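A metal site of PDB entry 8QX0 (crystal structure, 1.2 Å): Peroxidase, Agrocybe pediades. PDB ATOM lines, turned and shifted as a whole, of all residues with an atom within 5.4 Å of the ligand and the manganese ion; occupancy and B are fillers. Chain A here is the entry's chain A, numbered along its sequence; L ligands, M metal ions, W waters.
O2 of the ligand lies within salt-bridge range of NH1 of Arg 42 (3.3 Å). The backbone NH (N) of Asp 177 is in hydrogen-bond range of an oxygen (O1) of the ligand. An oxygen (O1) of the ligand lies within hydrogen-bond range of the backbone NH (N) of Asp 178, at 2.9 Å. An oxygen (O3) of the ligand is in hydrogen-bond range of the backbone NH (N) of Gly 175, at 3.0 Å. OD2 of Asp 178 sits close to O2 of the ligand, 2.6 Å away. FE1 of the ligand is bound by NE2 of His 171.
The backbone carbonyl oxygen (O) of Ala 174 sits at hydrogen-bond distance from the backbone NH (N) of Phe 188, 3.2 Å away. The backbone carbonyl oxygen of Val 173 lies within hydrogen-bond range of a ring nitrogen (ND1) of His 38 (3.0 Å). The backbone carbonyl oxygen of Ile 331 is in hydrogen-bond range of the side-chain amide nitrogen of Gln 333. The backbone NH (N) of Ser 232 is in hydrogen-bond range of the backbone carbonyl oxygen (O) of Pro 142 (2.9 Å). NH2 of Arg 42 is in hydrogen-bond range of O of Thr 78, 2.9 Å away. O of Val 166 lies within hydrogen-bond range of OG of Ser 170 (2.8 Å).
The backbone carbonyl oxygen (O) of Thr 78 sits close to an oxygen (O2) of the ligand (3.3 Å). His 38 touches the ligand (O to C31, 3.2 Å). O of Leu 41 touches C25 of the ligand, at 3.8 Å. CE2 of Phe 45 touches C3 of the ligand, 3.4 Å away. Pro 140 touches the ligand. C of Glu 141 touches C17 of the ligand, at 3.4 Å. Pro 142 touches the ligand. Ile 149 touches the ligand. Val 166 touches the ligand. Ile 167 touches the ligand (CD1 to C19, 3.7 Å). Ser 170 touches the ligand. Val 173 touches the ligand (O to C31, 3.9 Å). Ala 174 touches the ligand. CA of Ala 176 touches O1 of the ligand (3.8 Å). Ile 179 touches the ligand. Phe 188 touches the ligand. Leu 230 touches the ligand. Ser 232 touches the ligand (OG to C17, 3.8 Å). Ile 264 touches the ligand. Met 267 touches the ligand. Of the 34 residues printed, 26 come within 4 Å of the ligand. The nearest printed residue that does not touch the ligand is Gly 79 (4.1 Å).
Within 4 Å of the manganese ion: Asp 35, Asp 177 and Gln 333. Along chain A the residues within 4 Å of the manganese ion span positions 35 to 333.
The manganese ion is bound by the side-chain carboxylate (OD1) of Asp 35 (1.8 Å), the side-chain carboxylate (OD2) of Asp 177 (2.2 Å), an oxygen (O4) of the ligand (2.2 Å), water W2 (2.2 Å), water W7 (2.3 Å) and the side-chain amide oxygen (OE1) of Gln 333 (2.3 Å).
Water W7 lies within hydrogen-bond range of OD1 of Asp 177, O3 of the ligand and NE2 of Gln 333. Water W6 lies within hydrogen-bond range of O of Gly 175, N of Asp 177 and O2 of the ligand.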
ATOM      1  N   ASP A  35      -8.919 -15.416 -23.351  1.00  0.00           N
ATOM      2  CA  ASP A  35      -9.444 -14.254 -22.638  1.00  0.00           C
ATOM      3  C   ASP A  35      -8.324 -13.389 -22.039  1.00  0.00           C
ATOM      4  O   ASP A  35      -8.506 -12.188 -21.934  1.00  0.00           O
ATOM      5  CB  ASP A  35     -10.453 -14.659 -21.573  1.00  0.00           C
ATOM      6  CG  ASP A  35     -11.137 -13.474 -20.874  1.00  0.00           C
ATOM      7  OD1 ASP A  35     -11.887 -12.528 -21.419  1.00  0.00           O
ATOM      8  OD2 ASP A  35     -11.057 -13.521 -19.632  1.00  0.00           O
ATOM      9  N   HIS A  38      -7.249 -11.258 -24.839  1.00  0.00           N
ATOM     10  CA  HIS A  38      -8.253 -10.257 -25.164  1.00  0.00           C
ATOM     11  C   HIS A  38      -8.226  -9.143 -24.116  1.00  0.00           C
ATOM     12  O   HIS A  38      -8.360  -7.947 -24.436  1.00  0.00           O
ATOM     13  CB  HIS A  38      -9.647 -10.897 -25.166  1.00  0.00           C
ATOM     14  CG  HIS A  38      -9.796 -12.076 -26.084  1.00  0.00           C
ATOM     15  ND1 HIS A  38      -8.964 -12.341 -27.140  1.00  0.00           N
ATOM     16  CD2 HIS A  38     -10.636 -13.118 -26.027  1.00  0.00           C
ATOM     17  CE1 HIS A  38      -9.354 -13.457 -27.775  1.00  0.00           C
ATOM     18  NE2 HIS A  38     -10.341 -13.977 -27.090  1.00  0.00           N
ATOM     19  N   GLY A  39      -8.095  -9.496 -22.842  1.00  0.00           N
ATOM     20  CA  GLY A  39      -8.093  -8.501 -21.808  1.00  0.00           C
ATOM     21  C   GLY A  39      -6.889  -7.558 -21.939  1.00  0.00           C
ATOM     22  O   GLY A  39      -7.016  -6.369 -21.774  1.00  0.00           O
ATOM     23  N   LEU A  41      -5.284  -6.810 -24.654  1.00  0.00           N
ATOM     24  CA  LEU A  41      -5.527  -5.923 -25.787  1.00  0.00           C
ATOM     25  C   LEU A  41      -6.535  -4.834 -25.427  1.00  0.00           C
ATOM     26  O   LEU A  41      -6.314  -3.677 -25.783  1.00  0.00           O
ATOM     27  CB  LEU A  41      -5.979  -6.754 -26.998  1.00  0.00           C
ATOM     28  CG  LEU A  41      -6.268  -5.957 -28.268  1.00  0.00           C
ATOM     29  CD1 LEU A  41      -5.042  -5.171 -28.768  1.00  0.00           C
ATOM     30  CD2 LEU A  41      -6.780  -6.864 -29.365  1.00  0.00           C
ATOM     31  N   ARG A  42      -7.676  -5.162 -24.798  1.00  0.00           N
ATOM     32  CA  ARG A  42      -8.650  -4.164 -24.389  1.00  0.00           C
ATOM     33  C   ARG A  42      -7.966  -3.112 -23.526  1.00  0.00           C
ATOM     34  O   ARG A  42      -8.318  -1.933 -23.589  1.00  0.00           O
ATOM     35  CB  ARG A  42      -9.844  -4.862 -23.735  1.00  0.00           C
ATOM     36  CG  ARG A  42     -10.969  -3.899 -23.441  1.00  0.00           C
ATOM     37  CD  ARG A  42     -12.205  -4.620 -22.824  1.00  0.00           C
ATOM     38  NE  ARG A  42     -13.209  -3.624 -22.445  1.00  0.00           N
ATOM     39  CZ  ARG A  42     -13.987  -3.651 -21.400  1.00  0.00           C
ATOM     40  NH1 ARG A  42     -13.887  -4.644 -20.530  1.00  0.00           N
ATOM     41  NH2 ARG A  42     -14.831  -2.655 -21.186  1.00  0.00           N
ATOM     42  N   VAL A  44      -5.037  -1.897 -23.494  1.00  0.00           N
ATOM     43  CA  VAL A  44      -4.346  -0.883 -24.277  1.00  0.00           C
ATOM     44  C   VAL A  44      -5.267   0.292 -24.574  1.00  0.00           C
ATOM     45  O   VAL A  44      -4.887   1.468 -24.389  1.00  0.00           O
ATOM     46  CB  VAL A  44      -3.837  -1.514 -25.575  1.00  0.00           C
ATOM     47  CG1 VAL A  44      -3.419  -0.494 -26.641  1.00  0.00           C
ATOM     48  CG2 VAL A  44      -2.689  -2.459 -25.334  1.00  0.00           C
ATOM     49  N   PHE A  45      -6.470  -0.027 -25.087  1.00  0.00           N
ATOM     50  CA  PHE A  45      -7.437   1.007 -25.425  1.00  0.00           C
ATOM     51  C   PHE A  45      -7.864   1.816 -24.214  1.00  0.00           C
ATOM     52  O   PHE A  45      -7.885   3.034 -24.236  1.00  0.00           O
ATOM     53  CB  PHE A  45      -8.610   0.305 -26.112  1.00  0.00           C
ATOM     54  CG  PHE A  45      -9.735   1.208 -26.566  1.00  0.00           C
ATOM     55  CD1 PHE A  45      -9.470   2.319 -27.350  1.00  0.00           C
ATOM     56  CD2 PHE A  45     -11.028   0.964 -26.158  1.00  0.00           C
ATOM     57  CE1 PHE A  45     -10.526   3.110 -27.765  1.00  0.00           C
ATOM     58  CE2 PHE A  45     -12.079   1.807 -26.562  1.00  0.00           C
ATOM     59  CZ  PHE A  45     -11.779   2.860 -27.366  1.00  0.00           C
ATOM     60  N   THR A  78     -16.405  -0.675 -17.456  1.00  0.00           N
ATOM     61  CA  THR A  78     -17.019  -1.884 -16.933  1.00  0.00           C
ATOM     62  C   THR A  78     -16.222  -3.104 -17.413  1.00  0.00           C
ATOM     63  O   THR A  78     -15.907  -3.261 -18.586  1.00  0.00           O
ATOM     64  CB  THR A  78     -18.490  -1.951 -17.378  1.00  0.00           C
ATOM     65  OG1 THR A  78     -19.206  -0.853 -16.833  1.00  0.00           O
ATOM     66  CG2 THR A  78     -19.166  -3.223 -16.942  1.00  0.00           C
ATOM     67  N   GLY A  79     -15.929  -4.035 -16.506  1.00  0.00           N
ATOM     68  CA  GLY A  79     -15.238  -5.252 -16.869  1.00  0.00           C
ATOM     69  C   GLY A  79     -13.702  -5.155 -16.842  1.00  0.00           C
ATOM     70  O   GLY A  79     -13.003  -6.156 -16.872  1.00  0.00           O
ATOM     71  N   VAL A  83     -10.311  -7.790 -16.050  1.00  0.00           N
ATOM     72  CA  VAL A  83      -9.059  -7.799 -16.793  1.00  0.00           C
ATOM     73  C   VAL A  83      -7.876  -7.573 -15.842  1.00  0.00           C
ATOM     74  O   VAL A  83      -6.863  -8.269 -15.910  1.00  0.00           O
ATOM     75  CB  VAL A  83      -9.071  -6.728 -17.892  1.00  0.00           C
ATOM     76  CG1 VAL A  83      -7.697  -6.637 -18.558  1.00  0.00           C
ATOM     77  CG2 VAL A  83     -10.128  -7.024 -18.943  1.00  0.00           C
ATOM     78  N   PRO A 140     -14.732   5.922 -25.362  1.00  0.00           N
ATOM     79  CA  PRO A 140     -15.973   5.724 -26.102  1.00  0.00           C
ATOM     80  C   PRO A 140     -16.803   4.562 -25.608  1.00  0.00           C
ATOM     81  O   PRO A 140     -16.294   3.518 -25.202  1.00  0.00           O
ATOM     82  CB  PRO A 140     -15.463   5.465 -27.531  1.00  0.00           C
ATOM     83  CG  PRO A 140     -14.184   6.245 -27.614  1.00  0.00           C
ATOM     84  CD  PRO A 140     -13.553   6.000 -26.256  1.00  0.00           C
ATOM     85  N   GLU A 141     -18.122   4.763 -25.689  1.00  0.00           N
ATOM     86  CA  GLU A 141     -19.125   3.771 -25.315  1.00  0.00           C
ATOM     87  C   GLU A 141     -19.753   3.197 -26.551  1.00  0.00           C
ATOM     88  O   GLU A 141     -19.819   3.813 -27.603  1.00  0.00           O
ATOM     89  CB  GLU A 141     -20.220   4.516 -24.549  1.00  0.00           C
ATOM     90  CG  GLU A 141     -19.849   4.985 -23.137  1.00  0.00           C
ATOM     91  CD  GLU A 141     -20.035   3.954 -22.035  1.00  0.00           C
ATOM     92  OE1 GLU A 141     -20.187   2.788 -22.370  1.00  0.00           O
ATOM     93  OE2 GLU A 141     -20.057   4.373 -20.848  1.00  0.00           O
ATOM     94  N   PRO A 142     -20.336   1.981 -26.449  1.00  0.00           N
ATOM     95  CA  PRO A 142     -20.943   1.307 -27.583  1.00  0.00           C
ATOM     96  C   PRO A 142     -22.229   1.977 -28.069  1.00  0.00           C
ATOM     97  O   PRO A 142     -22.658   1.726 -29.207  1.00  0.00           O
ATOM     98  CB  PRO A 142     -21.206  -0.095 -27.111  1.00  0.00           C
ATOM     99  CG  PRO A 142     -21.283   0.016 -25.609  1.00  0.00           C
ATOM    100  CD  PRO A 142     -20.279   1.093 -25.270  1.00  0.00           C
ATOM    101  N   ILE A 149     -17.543   9.176 -32.112  1.00  0.00           N
ATOM    102  CA  ILE A 149     -16.397   8.296 -32.169  1.00  0.00           C
ATOM    103  C   ILE A 149     -15.349   8.936 -33.030  1.00  0.00           C
ATOM    104  O   ILE A 149     -14.170   8.930 -32.682  1.00  0.00           O
ATOM    105  CB  ILE A 149     -16.808   6.910 -32.680  1.00  0.00           C
ATOM    106  CG1 ILE A 149     -17.694   6.216 -31.627  1.00  0.00           C
ATOM    107  CG2 ILE A 149     -15.609   6.056 -33.073  1.00  0.00           C
ATOM    108  CD1 ILE A 149     -18.374   4.964 -32.111  1.00  0.00           C
ATOM    109  N   PHE A 153     -11.454   9.929 -31.869  1.00  0.00           N
ATOM    110  CA  PHE A 153     -10.270   9.400 -32.510  1.00  0.00           C
ATOM    111  C   PHE A 153      -9.605  10.455 -33.372  1.00  0.00           C
ATOM    112  O   PHE A 153      -8.366  10.552 -33.383  1.00  0.00           O
ATOM    113  CB  PHE A 153     -10.576   8.181 -33.341  1.00  0.00           C
ATOM    114  CG  PHE A 153     -10.754   6.888 -32.542  1.00  0.00           C
ATOM    115  CD1 PHE A 153     -11.918   6.577 -31.849  1.00  0.00           C
ATOM    116  CD2 PHE A 153      -9.753   5.934 -32.553  1.00  0.00           C
ATOM    117  CE1 PHE A 153     -12.022   5.374 -31.174  1.00  0.00           C
ATOM    118  CE2 PHE A 153      -9.851   4.769 -31.810  1.00  0.00           C
ATOM    119  CZ  PHE A 153     -11.004   4.453 -31.207  1.00  0.00           C
ATOM    120  N   VAL A 166      -8.681  -0.310 -36.199  1.00  0.00           N
ATOM    121  CA  VAL A 166      -8.278  -0.633 -34.828  1.00  0.00           C
ATOM    122  C   VAL A 166      -9.501  -1.152 -34.055  1.00  0.00           C
ATOM    123  O   VAL A 166      -9.361  -2.017 -33.211  1.00  0.00           O
ATOM    124  CB  VAL A 166      -7.491   0.490 -34.125  1.00  0.00           C
ATOM    125  CG1 VAL A 166      -8.366   1.620 -33.681  1.00  0.00           C
ATOM    126  CG2 VAL A 166      -6.577  -0.042 -33.008  1.00  0.00           C
ATOM    127  N   ILE A 167     -10.664  -0.570 -34.286  1.00  0.00           N
ATOM    128  CA  ILE A 167     -11.913  -1.010 -33.645  1.00  0.00           C
ATOM    129  C   ILE A 167     -12.291  -2.374 -34.191  1.00  0.00           C
ATOM    130  O   ILE A 167     -12.426  -3.330 -33.419  1.00  0.00           O
ATOM    131  CB  ILE A 167     -13.023   0.034 -33.761  1.00  0.00           C
ATOM    132  CG1 ILE A 167     -12.636   1.358 -33.185  1.00  0.00           C
ATOM    133  CG2 ILE A 167     -14.327  -0.486 -33.124  1.00  0.00           C
ATOM    134  CD1 ILE A 167     -13.577   2.497 -33.503  1.00  0.00           C
ATOM    135  N   SER A 170      -9.704  -5.223 -33.581  1.00  0.00           N
ATOM    136  CA  SER A 170      -9.706  -5.678 -32.208  1.00  0.00           C
ATOM    137  C   SER A 170     -10.880  -6.639 -31.968  1.00  0.00           C
ATOM    138  O   SER A 170     -10.769  -7.608 -31.208  1.00  0.00           O
ATOM    139  CB  SER A 170      -9.693  -4.582 -31.232  1.00  0.00           C
ATOM    140  OG  SER A 170      -8.440  -3.886 -31.267  1.00  0.00           O
ATOM    141  N   HIS A 171     -12.049  -6.281 -32.495  1.00  0.00           N
ATOM    142  CA  HIS A 171     -13.266  -7.024 -32.276  1.00  0.00           C
ATOM    143  C   HIS A 171     -13.280  -8.338 -33.019  1.00  0.00           C
ATOM    144  O   HIS A 171     -14.141  -9.159 -32.732  1.00  0.00           O
ATOM    145  CB  HIS A 171     -14.489  -6.119 -32.440  1.00  0.00           C
ATOM    146  CG  HIS A 171     -14.645  -5.091 -31.361  1.00  0.00           C
ATOM    147  ND1 HIS A 171     -15.628  -4.125 -31.346  1.00  0.00           N
ATOM    148  CD2 HIS A 171     -13.863  -4.782 -30.236  1.00  0.00           C
ATOM    149  CE1 HIS A 171     -15.410  -3.327 -30.305  1.00  0.00           C
ATOM    150  NE2 HIS A 171     -14.392  -3.719 -29.603  1.00  0.00           N
ATOM    151  N   VAL A 173     -11.014 -10.421 -32.287  1.00  0.00           N
ATOM    152  CA  VAL A 173     -10.391 -11.283 -31.307  1.00  0.00           C
ATOM    153  C   VAL A 173     -10.873 -10.838 -29.909  1.00  0.00           C
ATOM    154  O   VAL A 173     -10.114 -10.302 -29.076  1.00  0.00           O
ATOM    155  CB  VAL A 173      -8.854 -11.271 -31.441  1.00  0.00           C
ATOM    156  CG1 VAL A 173      -8.407 -12.092 -32.649  1.00  0.00           C
ATOM    157  CG2 VAL A 173      -8.268  -9.877 -31.475  1.00  0.00           C
ATOM    158  N   ALA A 174     -12.186 -11.029 -29.659  1.00  0.00           N
ATOM    159  CA  ALA A 174     -12.815 -10.326 -28.547  1.00  0.00           C
ATOM    160  C   ALA A 174     -14.191 -10.861 -28.259  1.00  0.00           C
ATOM    161  O   ALA A 174     -14.927 -11.300 -29.146  1.00  0.00           O
ATOM    162  CB  ALA A 174     -12.974  -8.852 -28.863  1.00  0.00           C
ATOM    163  N   GLY A 175     -14.552 -10.743 -26.978  1.00  0.00           N
ATOM    164  CA  GLY A 175     -15.927 -11.005 -26.598  1.00  0.00           C
ATOM    165  C   GLY A 175     -16.465  -9.993 -25.598  1.00  0.00           C
ATOM    166  O   GLY A 175     -15.711  -9.207 -24.993  1.00  0.00           O
ATOM    167  N   ALA A 176     -17.773 -10.046 -25.372  1.00  0.00           N
ATOM    168  CA  ALA A 176     -18.482  -9.156 -24.463  1.00  0.00           C
ATOM    169  C   ALA A 176     -18.842  -9.911 -23.202  1.00  0.00           C
ATOM    170  O   ALA A 176     -19.485 -10.983 -23.285  1.00  0.00           O
ATOM    171  CB  ALA A 176     -19.728  -8.639 -25.082  1.00  0.00           C
ATOM    172  N   ASP A 177     -18.435  -9.365 -22.074  1.00  0.00           N
ATOM    173  CA  ASP A 177     -18.599  -9.981 -20.762  1.00  0.00           C
ATOM    174  C   ASP A 177     -19.687  -9.336 -19.941  1.00  0.00           C
ATOM    175  O   ASP A 177     -20.138  -9.971 -18.961  1.00  0.00           O
ATOM    176  CB  ASP A 177     -17.261  -9.932 -20.058  1.00  0.00           C
ATOM    177  CG  ASP A 177     -16.163 -10.704 -20.762  1.00  0.00           C
ATOM    178  OD1 ASP A 177     -16.491 -11.577 -21.649  1.00  0.00           O
ATOM    179  OD2 ASP A 177     -14.989 -10.351 -20.465  1.00  0.00           O
ATOM    180  N   ASP A 178     -20.120  -8.137 -20.268  1.00  0.00           N
ATOM    181  CA  ASP A 178     -20.977  -7.283 -19.462  1.00  0.00           C
ATOM    182  C   ASP A 178     -22.110  -6.719 -20.318  1.00  0.00           C
ATOM    183  O   ASP A 178     -22.735  -5.710 -19.904  1.00  0.00           O
ATOM    184  CB  ASP A 178     -20.186  -6.191 -18.778  1.00  0.00           C
ATOM    185  CG  ASP A 178     -19.034  -6.735 -17.939  1.00  0.00           C
ATOM    186  OD1 ASP A 178     -19.337  -7.161 -16.781  1.00  0.00           O
ATOM    187  OD2 ASP A 178     -17.896  -6.876 -18.423  1.00  0.00           O
ATOM    188  N   ILE A 179     -22.410  -7.339 -21.441  1.00  0.00           N
ATOM    189  CA  ILE A 179     -23.481  -6.913 -22.331  1.00  0.00           C
ATOM    190  C   ILE A 179     -24.678  -7.861 -22.303  1.00  0.00           C
ATOM    191  O   ILE A 179     -25.806  -7.400 -22.124  1.00  0.00           O
ATOM    192  CB  ILE A 179     -22.946  -6.741 -23.759  1.00  0.00           C
ATOM    193  CG1 ILE A 179     -21.820  -5.697 -23.864  1.00  0.00           C
ATOM    194  CG2 ILE A 179     -24.080  -6.456 -24.736  1.00  0.00           C
ATOM    195  CD1 ILE A 179     -22.253  -4.278 -23.559  1.00  0.00           C
ATOM    196  N   PHE A 188     -17.751 -11.264 -30.568  1.00  0.00           N
ATOM    197  CA  PHE A 188     -18.252 -10.364 -31.578  1.00  0.00           C
ATOM    198  C   PHE A 188     -18.207 -10.963 -32.990  1.00  0.00           C
ATOM    199  O   PHE A 188     -19.039 -10.621 -33.838  1.00  0.00           O
ATOM    200  CB  PHE A 188     -17.486  -9.048 -31.622  1.00  0.00           C
ATOM    201  CG  PHE A 188     -17.553  -8.301 -30.292  1.00  0.00           C
ATOM    202  CD1 PHE A 188     -18.766  -7.857 -29.761  1.00  0.00           C
ATOM    203  CD2 PHE A 188     -16.385  -7.904 -29.640  1.00  0.00           C
ATOM    204  CE1 PHE A 188     -18.830  -7.168 -28.547  1.00  0.00           C
ATOM    205  CE2 PHE A 188     -16.442  -7.186 -28.468  1.00  0.00           C
ATOM    206  CZ  PHE A 188     -17.660  -6.820 -27.901  1.00  0.00           C
ATOM    207  N   LEU A 230     -22.338  -4.841 -31.153  1.00  0.00           N
ATOM    208  CA  LEU A 230     -22.382  -3.504 -30.570  1.00  0.00           C
ATOM    209  C   LEU A 230     -23.042  -2.575 -31.565  1.00  0.00           C
ATOM    210  O   LEU A 230     -22.762  -2.581 -32.774  1.00  0.00           O
ATOM    211  CB  LEU A 230     -20.961  -3.049 -30.272  1.00  0.00           C
ATOM    212  CG  LEU A 230     -20.184  -3.921 -29.297  1.00  0.00           C
ATOM    213  CD1 LEU A 230     -18.803  -3.348 -29.124  1.00  0.00           C
ATOM    214  CD2 LEU A 230     -20.858  -4.164 -27.961  1.00  0.00           C
ATOM    215  N   SER A 232     -22.177   0.564 -31.859  1.00  0.00           N
ATOM    216  CA  SER A 232     -21.078   1.300 -32.445  1.00  0.00           C
ATOM    217  C   SER A 232     -20.553   0.633 -33.706  1.00  0.00           C
ATOM    218  O   SER A 232     -20.340   1.256 -34.752  1.00  0.00           O
ATOM    219  CB  SER A 232     -19.972   1.546 -31.403  1.00  0.00           C
ATOM    220  OG  SER A 232     -19.689   0.325 -30.747  1.00  0.00           O
ATOM    221  N   LEU A 236     -20.760   1.943 -37.501  1.00  0.00           N
ATOM    222  CA  LEU A 236     -19.531   2.152 -38.255  1.00  0.00           C
ATOM    223  C   LEU A 236     -19.612   1.457 -39.628  1.00  0.00           C
ATOM    224  O   LEU A 236     -19.134   1.987 -40.623  1.00  0.00           O
ATOM    225  CB  LEU A 236     -18.281   1.708 -37.507  1.00  0.00           C
ATOM    226  CG  LEU A 236     -17.871   2.607 -36.337  1.00  0.00           C
ATOM    227  CD1 LEU A 236     -16.919   1.925 -35.367  1.00  0.00           C
ATOM    228  CD2 LEU A 236     -17.245   3.910 -36.883  1.00  0.00           C
ATOM    229  N   ILE A 264      -2.243   0.647 -33.658  1.00  0.00           N
ATOM    230  CA  ILE A 264      -1.891   0.285 -32.286  1.00  0.00           C
ATOM    231  C   ILE A 264      -0.636   1.056 -31.864  1.00  0.00           C
ATOM    232  O   ILE A 264      -0.549   1.553 -30.752  1.00  0.00           O
ATOM    233  CB  ILE A 264      -1.689  -1.230 -32.173  1.00  0.00           C
ATOM    234  CG1 ILE A 264      -3.012  -1.991 -32.296  1.00  0.00           C
ATOM    235  CG2 ILE A 264      -0.965  -1.634 -30.871  1.00  0.00           C
ATOM    236  CD1 ILE A 264      -3.982  -1.851 -31.121  1.00  0.00           C
ATOM    237  N   MET A 267      -1.565   4.498 -31.081  1.00  0.00           N
ATOM    238  CA  MET A 267      -2.277   4.540 -29.811  1.00  0.00           C
ATOM    239  C   MET A 267      -1.303   4.452 -28.627  1.00  0.00           C
ATOM    240  O   MET A 267      -1.528   5.093 -27.608  1.00  0.00           O
ATOM    241  CB  MET A 267      -3.263   3.369 -29.836  1.00  0.00           C
ATOM    242  CG  MET A 267      -4.225   3.327 -28.688  1.00  0.00           C
ATOM    243  SD  MET A 267      -5.584   2.161 -28.800  1.00  0.00           S
ATOM    244  CE  MET A 267      -6.493   2.857 -30.185  1.00  0.00           C
ATOM    245  N   ILE A 331     -16.280 -17.820 -24.891  1.00  0.00           N
ATOM    246  CA  ILE A 331     -14.870 -17.750 -24.541  1.00  0.00           C
ATOM    247  C   ILE A 331     -14.736 -17.991 -23.046  1.00  0.00           C
ATOM    248  O   ILE A 331     -15.286 -17.246 -22.244  1.00  0.00           O
ATOM    249  CB  ILE A 331     -14.284 -16.335 -24.849  1.00  0.00           C
ATOM    250  CG1 ILE A 331     -14.461 -15.980 -26.317  1.00  0.00           C
ATOM    251  CG2 ILE A 331     -12.825 -16.270 -24.438  1.00  0.00           C
ATOM    252  CD1 ILE A 331     -14.385 -14.494 -26.581  1.00  0.00           C
ATOM    253  N   GLN A 333     -13.388 -17.590 -19.439  1.00  0.00           N
ATOM    254  CA  GLN A 333     -12.795 -16.388 -18.875  1.00  0.00           C
ATOM    255  C   GLN A 333     -11.560 -16.733 -18.056  1.00  0.00           C
ATOM    256  O   GLN A 333     -11.559 -17.740 -17.327  1.00  0.00           O
ATOM    257  CB  GLN A 333     -13.900 -15.657 -18.137  1.00  0.00           C
ATOM    258  CG  GLN A 333     -15.005 -15.124 -19.038  1.00  0.00           C
ATOM    259  CD  GLN A 333     -14.459 -14.171 -20.109  1.00  0.00           C
ATOM    260  OE1 GLN A 333     -14.100 -13.017 -19.805  1.00  0.00           O
ATOM    261  NE2 GLN A 333     -14.424 -14.634 -21.332  1.00  0.00           N
HETATM  262  C1  LIG L   1     -14.594  -5.521 -25.826  1.00  0.00           C
HETATM  263  C2  LIG L   1     -16.602  -1.288 -27.044  1.00  0.00           C
HETATM  264  C3  LIG L   1     -12.578  -0.040 -29.396  1.00  0.00           C
HETATM  265  C4  LIG L   1     -10.456  -4.056 -27.789  1.00  0.00           C
HETATM  266  C5  LIG L   1     -15.481  -4.449 -25.886  1.00  0.00           C
HETATM  267  C6  LIG L   1     -16.764  -4.366 -25.267  1.00  0.00           C
HETATM  268  C7  LIG L   1     -17.338  -3.204 -25.575  1.00  0.00           C
HETATM  269  C8  LIG L   1     -16.398  -2.508 -26.429  1.00  0.00           C
HETATM  270  C9  LIG L   1     -18.672  -2.607 -25.098  1.00  0.00           C
HETATM  271  C10 LIG L   1     -17.341  -5.338 -24.264  1.00  0.00           C
HETATM  272  C11 LIG L   1     -16.883  -4.956 -22.800  1.00  0.00           C
HETATM  273  C12 LIG L   1     -17.562  -5.689 -21.729  1.00  0.00           C
HETATM  274  O1  LIG L   1     -18.655  -6.304 -21.924  1.00  0.00           O
HETATM  275  O2  LIG L   1     -16.966  -5.718 -20.560  1.00  0.00           O
HETATM  276  C13 LIG L   1     -15.719  -0.546 -27.845  1.00  0.00           C
HETATM  277  C14 LIG L   1     -16.011   0.746 -28.404  1.00  0.00           C
HETATM  278  C15 LIG L   1     -14.868   1.081 -29.105  1.00  0.00           C
HETATM  279  C16 LIG L   1     -13.934  -0.056 -28.959  1.00  0.00           C
HETATM  280  C17 LIG L   1     -17.219   1.568 -28.209  1.00  0.00           C
HETATM  281  C18 LIG L   1     -14.545   2.277 -29.893  1.00  0.00           C
HETATM  282  C19 LIG L   1     -15.426   3.183 -30.428  1.00  0.00           C
HETATM  283  C20 LIG L   1     -11.583  -1.000 -29.152  1.00  0.00           C
HETATM  284  C21 LIG L   1     -10.184  -0.847 -29.395  1.00  0.00           C
HETATM  285  C22 LIG L   1      -9.542  -1.927 -28.905  1.00  0.00           C
HETATM  286  C23 LIG L   1     -10.598  -2.808 -28.327  1.00  0.00           C
HETATM  287  C24 LIG L   1      -9.571   0.263 -30.182  1.00  0.00           C
HETATM  288  C25 LIG L   1      -8.108  -2.259 -28.825  1.00  0.00           C
HETATM  289  C26 LIG L   1      -7.113  -1.450 -29.062  1.00  0.00           C
HETATM  290  C27 LIG L   1     -11.434  -4.868 -27.243  1.00  0.00           C
HETATM  291  C28 LIG L   1     -11.154  -6.237 -26.820  1.00  0.00           C
HETATM  292  C29 LIG L   1     -12.341  -6.602 -26.280  1.00  0.00           C
HETATM  293  C30 LIG L   1     -13.261  -5.473 -26.305  1.00  0.00           C
HETATM  294  C31 LIG L   1      -9.965  -7.016 -27.036  1.00  0.00           C
HETATM  295  C32 LIG L   1     -12.640  -7.968 -25.658  1.00  0.00           C
HETATM  296  C33 LIG L   1     -12.361  -8.167 -24.190  1.00  0.00           C
HETATM  297  C34 LIG L   1     -12.664  -9.589 -23.661  1.00  0.00           C
HETATM  298  O3  LIG L   1     -12.866 -10.490 -24.461  1.00  0.00           O
HETATM  299  O4  LIG L   1     -12.652  -9.713 -22.425  1.00  0.00           O
HETATM  300  N1  LIG L   1     -15.300  -3.285 -26.626  1.00  0.00           N
HETATM  301  N2  LIG L   1     -14.505  -1.041 -28.133  1.00  0.00           N
HETATM  302  N3  LIG L   1     -11.831  -2.157 -28.390  1.00  0.00           N
HETATM  303  N4  LIG L   1     -12.673  -4.421 -26.947  1.00  0.00           N
HETATM  304 FE1  LIG L   1     -13.650  -2.855 -27.812  1.00  0.00          FE
HETATM  305 MN    MN M   1     -13.183 -11.377 -21.115  1.00  0.00          MN
HETATM  306  O   HOH W   1     -15.248  -1.153 -23.834  1.00  0.00           O
HETATM  307  O   HOH W   2     -12.220 -10.370 -19.414  1.00  0.00           O
HETATM  308  O   HOH W   3     -13.446  -7.446 -21.008  1.00  0.00           O
HETATM  309  O   HOH W   4     -17.191  -0.380 -31.268  1.00  0.00           O
HETATM  310  O   HOH W   5     -16.732   0.930 -24.474  1.00  0.00           O
HETATM  311  O   HOH W   6     -15.863  -7.978 -22.559  1.00  0.00           O
HETATM  312  O   HOH W   7     -14.236 -12.269 -22.929  1.00  0.00           O
